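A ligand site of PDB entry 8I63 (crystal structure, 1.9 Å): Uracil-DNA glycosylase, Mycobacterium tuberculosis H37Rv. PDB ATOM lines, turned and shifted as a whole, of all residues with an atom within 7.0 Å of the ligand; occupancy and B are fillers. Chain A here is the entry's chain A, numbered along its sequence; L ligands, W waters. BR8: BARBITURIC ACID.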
ATOM      1  N   VAL A  76       9.456  32.357 -14.949  1.00  0.00           N
ATOM      2  CA  VAL A  76       8.096  31.929 -15.297  1.00  0.00           C
ATOM      3  C   VAL A  76       8.169  30.501 -15.796  1.00  0.00           C
ATOM      4  O   VAL A  76       8.857  30.268 -16.796  1.00  0.00           O
ATOM      5  CB  VAL A  76       7.487  32.862 -16.371  1.00  0.00           C
ATOM      6  CG1 VAL A  76       6.024  32.482 -16.652  1.00  0.00           C
ATOM      7  CG2 VAL A  76       7.599  34.323 -15.956  1.00  0.00           C
ATOM      8  N   GLY A  77       7.430  29.609 -15.160  1.00  0.00           N
ATOM      9  CA  GLY A  77       7.104  28.268 -15.686  1.00  0.00           C
ATOM     10  C   GLY A  77       5.669  28.182 -16.150  1.00  0.00           C
ATOM     11  O   GLY A  77       4.969  29.232 -16.140  1.00  0.00           O
ATOM     12  N   GLN A  78       5.184  27.000 -16.499  1.00  0.00           N
ATOM     13  CA  GLN A  78       3.811  26.891 -17.072  1.00  0.00           C
ATOM     14  C   GLN A  78       2.878  26.309 -15.990  1.00  0.00           C
ATOM     15  O   GLN A  78       2.019  27.075 -15.490  1.00  0.00           O
ATOM     16  CB  GLN A  78       3.845  26.192 -18.432  1.00  0.00           C
ATOM     17  CG  GLN A  78       2.478  26.121 -19.137  1.00  0.00           C
ATOM     18  CD  GLN A  78       1.616  27.381 -19.201  1.00  0.00           C
ATOM     19  OE1 GLN A  78       0.456  27.357 -18.811  1.00  0.00           O
ATOM     20  NE2 GLN A  78       2.167  28.488 -19.714  1.00  0.00           N
ATOM     21  N   ASP A  79       3.083  25.039 -15.627  1.00  0.00           N
ATOM     22  CA  ASP A  79       2.274  24.258 -14.665  1.00  0.00           C
ATOM     23  C   ASP A  79       3.174  23.626 -13.610  1.00  0.00           C
ATOM     24  O   ASP A  79       4.328  23.326 -13.887  1.00  0.00           O
ATOM     25  CB  ASP A  79       1.526  23.104 -15.329  1.00  0.00           C
ATOM     26  CG  ASP A  79       0.665  23.553 -16.473  1.00  0.00           C
ATOM     27  OD1 ASP A  79      -0.496  23.992 -16.200  1.00  0.00           O
ATOM     28  OD2 ASP A  79       1.162  23.480 -17.615  1.00  0.00           O
ATOM     29  N   PRO A  80       2.638  23.297 -12.414  1.00  0.00           N
ATOM     30  CA  PRO A  80       3.383  22.520 -11.430  1.00  0.00           C
ATOM     31  C   PRO A  80       3.731  21.134 -12.007  1.00  0.00           C
ATOM     32  O   PRO A  80       3.056  20.608 -12.908  1.00  0.00           O
ATOM     33  CB  PRO A  80       2.449  22.455 -10.210  1.00  0.00           C
ATOM     34  CG  PRO A  80       1.457  23.580 -10.434  1.00  0.00           C
ATOM     35  CD  PRO A  80       1.286  23.633 -11.940  1.00  0.00           C
ATOM     36  N   TYR A  81       4.801  20.543 -11.483  1.00  0.00           N
ATOM     37  CA  TYR A  81       5.117  19.109 -11.674  1.00  0.00           C
ATOM     38  C   TYR A  81       3.849  18.305 -11.442  1.00  0.00           C
ATOM     39  O   TYR A  81       3.184  18.467 -10.415  1.00  0.00           O
ATOM     40  CB  TYR A  81       6.216  18.629 -10.744  1.00  0.00           C
ATOM     41  CG  TYR A  81       7.588  19.181 -11.033  1.00  0.00           C
ATOM     42  CD1 TYR A  81       8.278  18.866 -12.206  1.00  0.00           C
ATOM     43  CD2 TYR A  81       8.264  19.930 -10.069  1.00  0.00           C
ATOM     44  CE1 TYR A  81       9.562  19.344 -12.432  1.00  0.00           C
ATOM     45  CE2 TYR A  81       9.550  20.372 -10.266  1.00  0.00           C
ATOM     46  CZ  TYR A  81      10.203  20.081 -11.450  1.00  0.00           C
ATOM     47  OH  TYR A  81      11.465  20.588 -11.607  1.00  0.00           O
ATOM     48  N   PRO A  82       3.486  17.412 -12.387  1.00  0.00           N
ATOM     49  CA  PRO A  82       2.316  16.559 -12.231  1.00  0.00           C
ATOM     50  C   PRO A  82       2.574  15.280 -11.425  1.00  0.00           C
ATOM     51  O   PRO A  82       1.601  14.638 -11.063  1.00  0.00           O
ATOM     52  CB  PRO A  82       1.964  16.201 -13.687  1.00  0.00           C
ATOM     53  CG  PRO A  82       3.304  16.172 -14.373  1.00  0.00           C
ATOM     54  CD  PRO A  82       4.156  17.224 -13.676  1.00  0.00           C
ATOM     55  N   ALA A  87       5.886  18.914  -6.958  1.00  0.00           N
ATOM     56  CA  ALA A  87       5.418  20.316  -6.885  1.00  0.00           C
ATOM     57  C   ALA A  87       5.465  20.797  -5.437  1.00  0.00           C
ATOM     58  O   ALA A  87       4.877  20.109  -4.565  1.00  0.00           O
ATOM     59  CB  ALA A  87       4.035  20.418  -7.476  1.00  0.00           C
ATOM     60  N   LEU A  90       6.847  26.480  -5.737  1.00  0.00           N
ATOM     61  CA  LEU A  90       7.892  27.276  -6.425  1.00  0.00           C
ATOM     62  C   LEU A  90       8.188  26.567  -7.738  1.00  0.00           C
ATOM     63  O   LEU A  90       8.515  25.364  -7.694  1.00  0.00           O
ATOM     64  CB  LEU A  90       9.126  27.343  -5.531  1.00  0.00           C
ATOM     65  CG  LEU A  90       8.958  27.925  -4.125  1.00  0.00           C
ATOM     66  CD1 LEU A  90      10.288  27.935  -3.392  1.00  0.00           C
ATOM     67  CD2 LEU A  90       8.383  29.349  -4.166  1.00  0.00           C
ATOM     68  N   SER A  91       8.087  27.251  -8.862  1.00  0.00           N
ATOM     69  CA  SER A  91       8.383  26.688 -10.205  1.00  0.00           C
ATOM     70  C   SER A  91       9.746  25.989 -10.178  1.00  0.00           C
ATOM     71  O   SER A  91      10.690  26.546  -9.595  1.00  0.00           O
ATOM     72  CB  SER A  91       8.280  27.741 -11.304  1.00  0.00           C
ATOM     73  OG  SER A  91       9.190  28.806 -11.109  1.00  0.00           O
ATOM     74  N   PHE A  92       9.759  24.748 -10.668  1.00  0.00           N
ATOM     75  CA  PHE A  92      10.954  23.897 -10.915  1.00  0.00           C
ATOM     76  C   PHE A  92      11.496  23.289  -9.627  1.00  0.00           C
ATOM     77  O   PHE A  92      12.185  22.287  -9.742  1.00  0.00           O
ATOM     78  CB  PHE A  92      12.029  24.659 -11.686  1.00  0.00           C
ATOM     79  CG  PHE A  92      11.533  25.134 -13.032  1.00  0.00           C
ATOM     80  CD1 PHE A  92      11.349  24.234 -14.073  1.00  0.00           C
ATOM     81  CD2 PHE A  92      11.194  26.461 -13.230  1.00  0.00           C
ATOM     82  CE1 PHE A  92      10.855  24.667 -15.301  1.00  0.00           C
ATOM     83  CE2 PHE A  92      10.673  26.886 -14.445  1.00  0.00           C
ATOM     84  CZ  PHE A  92      10.506  25.984 -15.480  1.00  0.00           C
ATOM     85  N   SER A  93      11.232  23.861  -8.454  1.00  0.00           N
ATOM     86  CA  SER A  93      11.819  23.390  -7.179  1.00  0.00           C
ATOM     87  C   SER A  93      11.244  22.027  -6.814  1.00  0.00           C
ATOM     88  O   SER A  93      10.095  21.706  -7.228  1.00  0.00           O
ATOM     89  CB  SER A  93      11.618  24.391  -6.054  1.00  0.00           C
ATOM     90  OG  SER A  93      12.336  23.980  -4.902  1.00  0.00           O
ATOM     91  N   PRO A 102      13.714  15.793 -11.220  1.00  0.00           N
ATOM     92  CA  PRO A 102      13.037  15.880 -12.511  1.00  0.00           C
ATOM     93  C   PRO A 102      13.965  16.390 -13.621  1.00  0.00           C
ATOM     94  O   PRO A 102      14.828  17.227 -13.337  1.00  0.00           O
ATOM     95  CB  PRO A 102      11.928  16.921 -12.283  1.00  0.00           C
ATOM     96  CG  PRO A 102      11.695  16.879 -10.788  1.00  0.00           C
ATOM     97  CD  PRO A 102      13.043  16.560 -10.171  1.00  0.00           C
ATOM     98  N   ARG A 103      13.758  15.920 -14.861  1.00  0.00           N
ATOM     99  CA  ARG A 103      14.572  16.265 -16.066  1.00  0.00           C
ATOM    100  C   ARG A 103      14.755  17.797 -16.181  1.00  0.00           C
ATOM    101  O   ARG A 103      15.890  18.275 -16.433  1.00  0.00           O
ATOM    102  CB  ARG A 103      13.871  15.710 -17.313  1.00  0.00           C
ATOM    103  CG  ARG A 103      14.815  15.096 -18.332  1.00  0.00           C
ATOM    104  CD  ARG A 103      14.425  15.302 -19.800  1.00  0.00           C
ATOM    105  NE  ARG A 103      15.625  15.607 -20.584  1.00  0.00           N
ATOM    106  CZ  ARG A 103      15.801  16.634 -21.431  1.00  0.00           C
ATOM    107  NH1 ARG A 103      16.976  16.778 -22.029  1.00  0.00           N
ATOM    108  NH2 ARG A 103      14.842  17.507 -21.673  1.00  0.00           N
ATOM    109  N   SER A 104      13.697  18.573 -15.975  1.00  0.00           N
ATOM    110  CA  SER A 104      13.744  20.045 -16.165  1.00  0.00           C
ATOM    111  C   SER A 104      14.751  20.640 -15.186  1.00  0.00           C
ATOM    112  O   SER A 104      15.584  21.483 -15.619  1.00  0.00           O
ATOM    113  CB  SER A 104      12.391  20.679 -16.017  1.00  0.00           C
ATOM    114  OG  SER A 104      11.611  20.400 -17.156  1.00  0.00           O
ATOM    115  N   LEU A 105      14.712  20.179 -13.939  1.00  0.00           N
ATOM    116  CA  LEU A 105      15.598  20.725 -12.877  1.00  0.00           C
ATOM    117  C   LEU A 105      17.047  20.268 -13.112  1.00  0.00           C
ATOM    118  O   LEU A 105      17.963  21.115 -12.985  1.00  0.00           O
ATOM    119  CB  LEU A 105      15.026  20.336 -11.510  1.00  0.00           C
ATOM    120  CG  LEU A 105      15.779  20.905 -10.320  1.00  0.00           C
ATOM    121  CD1 LEU A 105      15.772  22.428 -10.376  1.00  0.00           C
ATOM    122  CD2 LEU A 105      15.222  20.398  -9.001  1.00  0.00           C
ATOM    123  N   LEU A 137       7.645  31.572 -10.491  1.00  0.00           N
ATOM    124  CA  LEU A 137       6.185  31.659 -10.737  1.00  0.00           C
ATOM    125  C   LEU A 137       5.776  30.751 -11.902  1.00  0.00           C
ATOM    126  O   LEU A 137       6.178  31.011 -13.039  1.00  0.00           O
ATOM    127  CB  LEU A 137       5.790  33.108 -11.002  1.00  0.00           C
ATOM    128  CG  LEU A 137       4.272  33.342 -11.144  1.00  0.00           C
ATOM    129  CD1 LEU A 137       3.577  33.175  -9.815  1.00  0.00           C
ATOM    130  CD2 LEU A 137       3.991  34.710 -11.738  1.00  0.00           C
ATOM    131  N   ASN A 138       4.913  29.791 -11.620  1.00  0.00           N
ATOM    132  CA  ASN A 138       4.122  29.067 -12.663  1.00  0.00           C
ATOM    133  C   ASN A 138       2.922  29.924 -13.066  1.00  0.00           C
ATOM    134  O   ASN A 138       2.283  30.592 -12.175  1.00  0.00           O
ATOM    135  CB  ASN A 138       3.711  27.681 -12.152  1.00  0.00           C
ATOM    136  CG  ASN A 138       4.852  26.695 -12.183  1.00  0.00           C
ATOM    137  OD1 ASN A 138       5.624  26.707 -13.137  1.00  0.00           O
ATOM    138  ND2 ASN A 138       4.966  25.859 -11.155  1.00  0.00           N
ATOM    139  N   ARG A 139       2.596  29.931 -14.354  1.00  0.00           N
ATOM    140  CA  ARG A 139       1.407  30.647 -14.865  1.00  0.00           C
ATOM    141  C   ARG A 139       0.143  30.058 -14.238  1.00  0.00           C
ATOM    142  O   ARG A 139      -0.807  30.833 -14.033  1.00  0.00           O
ATOM    143  CB  ARG A 139       1.273  30.557 -16.390  1.00  0.00           C
ATOM    144  CG  ARG A 139       2.042  31.600 -17.190  1.00  0.00           C
ATOM    145  CD  ARG A 139       2.006  33.084 -16.796  1.00  0.00           C
ATOM    146  NE  ARG A 139       0.729  33.730 -16.450  1.00  0.00           N
ATOM    147  CZ  ARG A 139      -0.310  33.966 -17.267  1.00  0.00           C
ATOM    148  NH1 ARG A 139      -1.375  34.575 -16.803  1.00  0.00           N
ATOM    149  NH2 ARG A 139      -0.270  33.603 -18.555  1.00  0.00           N
ATOM    150  N   TRP A 179      10.820  30.580 -19.059  1.00  0.00           N
ATOM    151  CA  TRP A 179      11.043  29.111 -19.270  1.00  0.00           C
ATOM    152  C   TRP A 179       9.708  28.375 -19.454  1.00  0.00           C
ATOM    153  O   TRP A 179       9.649  27.197 -19.111  1.00  0.00           O
ATOM    154  CB  TRP A 179      11.829  28.492 -18.114  1.00  0.00           C
ATOM    155  CG  TRP A 179      13.272  28.897 -18.028  1.00  0.00           C
ATOM    156  CD1 TRP A 179      14.047  29.451 -18.995  1.00  0.00           C
ATOM    157  CD2 TRP A 179      14.124  28.731 -16.883  1.00  0.00           C
ATOM    158  NE1 TRP A 179      15.311  29.675 -18.521  1.00  0.00           N
ATOM    159  CE2 TRP A 179      15.388  29.239 -17.229  1.00  0.00           C
ATOM    160  CE3 TRP A 179      13.938  28.160 -15.629  1.00  0.00           C
ATOM    161  CZ2 TRP A 179      16.457  29.223 -16.348  1.00  0.00           C
ATOM    162  CZ3 TRP A 179      14.991  28.168 -14.747  1.00  0.00           C
ATOM    163  CH2 TRP A 179      16.230  28.698 -15.109  1.00  0.00           C
ATOM    164  N   GLY A 180       8.689  29.037 -19.992  1.00  0.00           N
ATOM    165  CA  GLY A 180       7.358  28.455 -20.265  1.00  0.00           C
ATOM    166  C   GLY A 180       6.850  28.676 -21.686  1.00  0.00           C
ATOM    167  O   GLY A 180       5.623  28.516 -21.869  1.00  0.00           O
ATOM    168  N   PRO A 205      14.049  24.693 -20.247  1.00  0.00           N
ATOM    169  CA  PRO A 205      14.997  23.679 -19.795  1.00  0.00           C
ATOM    170  C   PRO A 205      14.956  22.350 -20.564  1.00  0.00           C
ATOM    171  O   PRO A 205      16.014  21.775 -20.734  1.00  0.00           O
ATOM    172  CB  PRO A 205      14.588  23.476 -18.336  1.00  0.00           C
ATOM    173  CG  PRO A 205      14.057  24.800 -17.923  1.00  0.00           C
ATOM    174  CD  PRO A 205      13.312  25.294 -19.136  1.00  0.00           C
ATOM    175  N   LEU A 206      13.801  21.885 -21.023  1.00  0.00           N
ATOM    176  CA  LEU A 206      13.697  20.666 -21.888  1.00  0.00           C
ATOM    177  C   LEU A 206      14.118  20.949 -23.346  1.00  0.00           C
ATOM    178  O   LEU A 206      14.257  19.966 -24.106  1.00  0.00           O
ATOM    179  CB  LEU A 206      12.280  20.099 -21.819  1.00  0.00           C
ATOM    180  CG  LEU A 206      11.730  19.748 -20.436  1.00  0.00           C
ATOM    181  CD1 LEU A 206      10.376  19.069 -20.558  1.00  0.00           C
ATOM    182  CD2 LEU A 206      12.687  18.871 -19.630  1.00  0.00           C
HETATM  183  N1  BR8 L   1       7.235  24.537 -14.115  1.00  0.00           N
HETATM  184  C2  BR8 L   1       7.488  23.684 -13.074  1.00  0.00           C
HETATM  185  O2  BR8 L   1       7.239  23.955 -11.912  1.00  0.00           O
HETATM  186  N3  BR8 L   1       8.050  22.471 -13.413  1.00  0.00           N
HETATM  187  C4  BR8 L   1       8.343  22.058 -14.697  1.00  0.00           C
HETATM  188  O4  BR8 L   1       8.944  21.016 -14.900  1.00  0.00           O
HETATM  189  C5  BR8 L   1       7.891  22.918 -15.821  1.00  0.00           C
HETATM  190  C6  BR8 L   1       7.264  24.218 -15.440  1.00  0.00           C
HETATM  191  O8  BR8 L   1       6.784  24.933 -16.291  1.00  0.00           O
HETATM  192  O   HOH W   1       8.286  25.159 -18.597  1.00  0.00           O
HETATM  193  O   HOH W   2       6.810  19.447 -15.319  1.00  0.00           O
HETATM  194  O   HOH W   3       6.267  22.661  -9.608  1.00  0.00           O
HETATM  195  O   HOH W   4       4.993  21.346 -15.501  1.00  0.00           O
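The backbone carbonyl oxygen (O) of Asp 79 is in hydrogen-bond range of a nitrogen (N1) of the ligand. A nitrogen (N1) of the ligand sits at hydrogen-bond distance from the side-chain amide oxygen (OD1) of Asn 138, 2.9 Å away. The backbone NH (N) of Gln 78 lies within hydrogen-bond range of an oxygen (O8) of the ligand, at 2.6 Å. The backbone NH (N) of Phe 92 is in hydrogen-bond range of an oxygen (O2) of the ligand.
O of Leu 137 sits at hydrogen-bond distance from N of Gly 77 (2.8 Å). The backbone NH (N) of Arg 139 is in hydrogen-bond range of the backbone carbonyl oxygen (O) of Gln 78 (3.1 Å). OG of Ser 91 sits at hydrogen-bond distance from N of Leu 137 (3.2 Å). The side-chain amide oxygen (OD1) of Asn 138 is in hydrogen-bond range of the backbone NH (N) of Gln 78 (3.4 Å). The side-chain hydroxyl (OH) of Tyr 81 is in hydrogen-bond range of the backbone carbonyl oxygen (O) of Phe 92 (2.6 Å). O of Gly 77 lies within hydrogen-bond range of N of Arg 139 (3.1 Å).
Water W1 lies within hydrogen-bond range of the backbone carbonyl oxygen of Trp 179 and an oxygen (O8) of the ligand. Water W3 bridges an oxygen (O2) of the ligand (2.8 Å) and the backbone NH of Tyr 81 (3.2 Å).
Residues that only touch the ligand: Gly 77 (3.4 Å), Tyr 81 (3.0 Å), Ser 91 (3.4 Å) and Ser 104 (3.5 Å). Hydrophobic or aromatic side chains within 4 Å of the ligand: Tyr 81 and Phe 92. Of the 23 residues printed, 8 come within 4 Å of the ligand. The nearest printed residue that does not touch the ligand is Pro 80 (4.1 Å).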
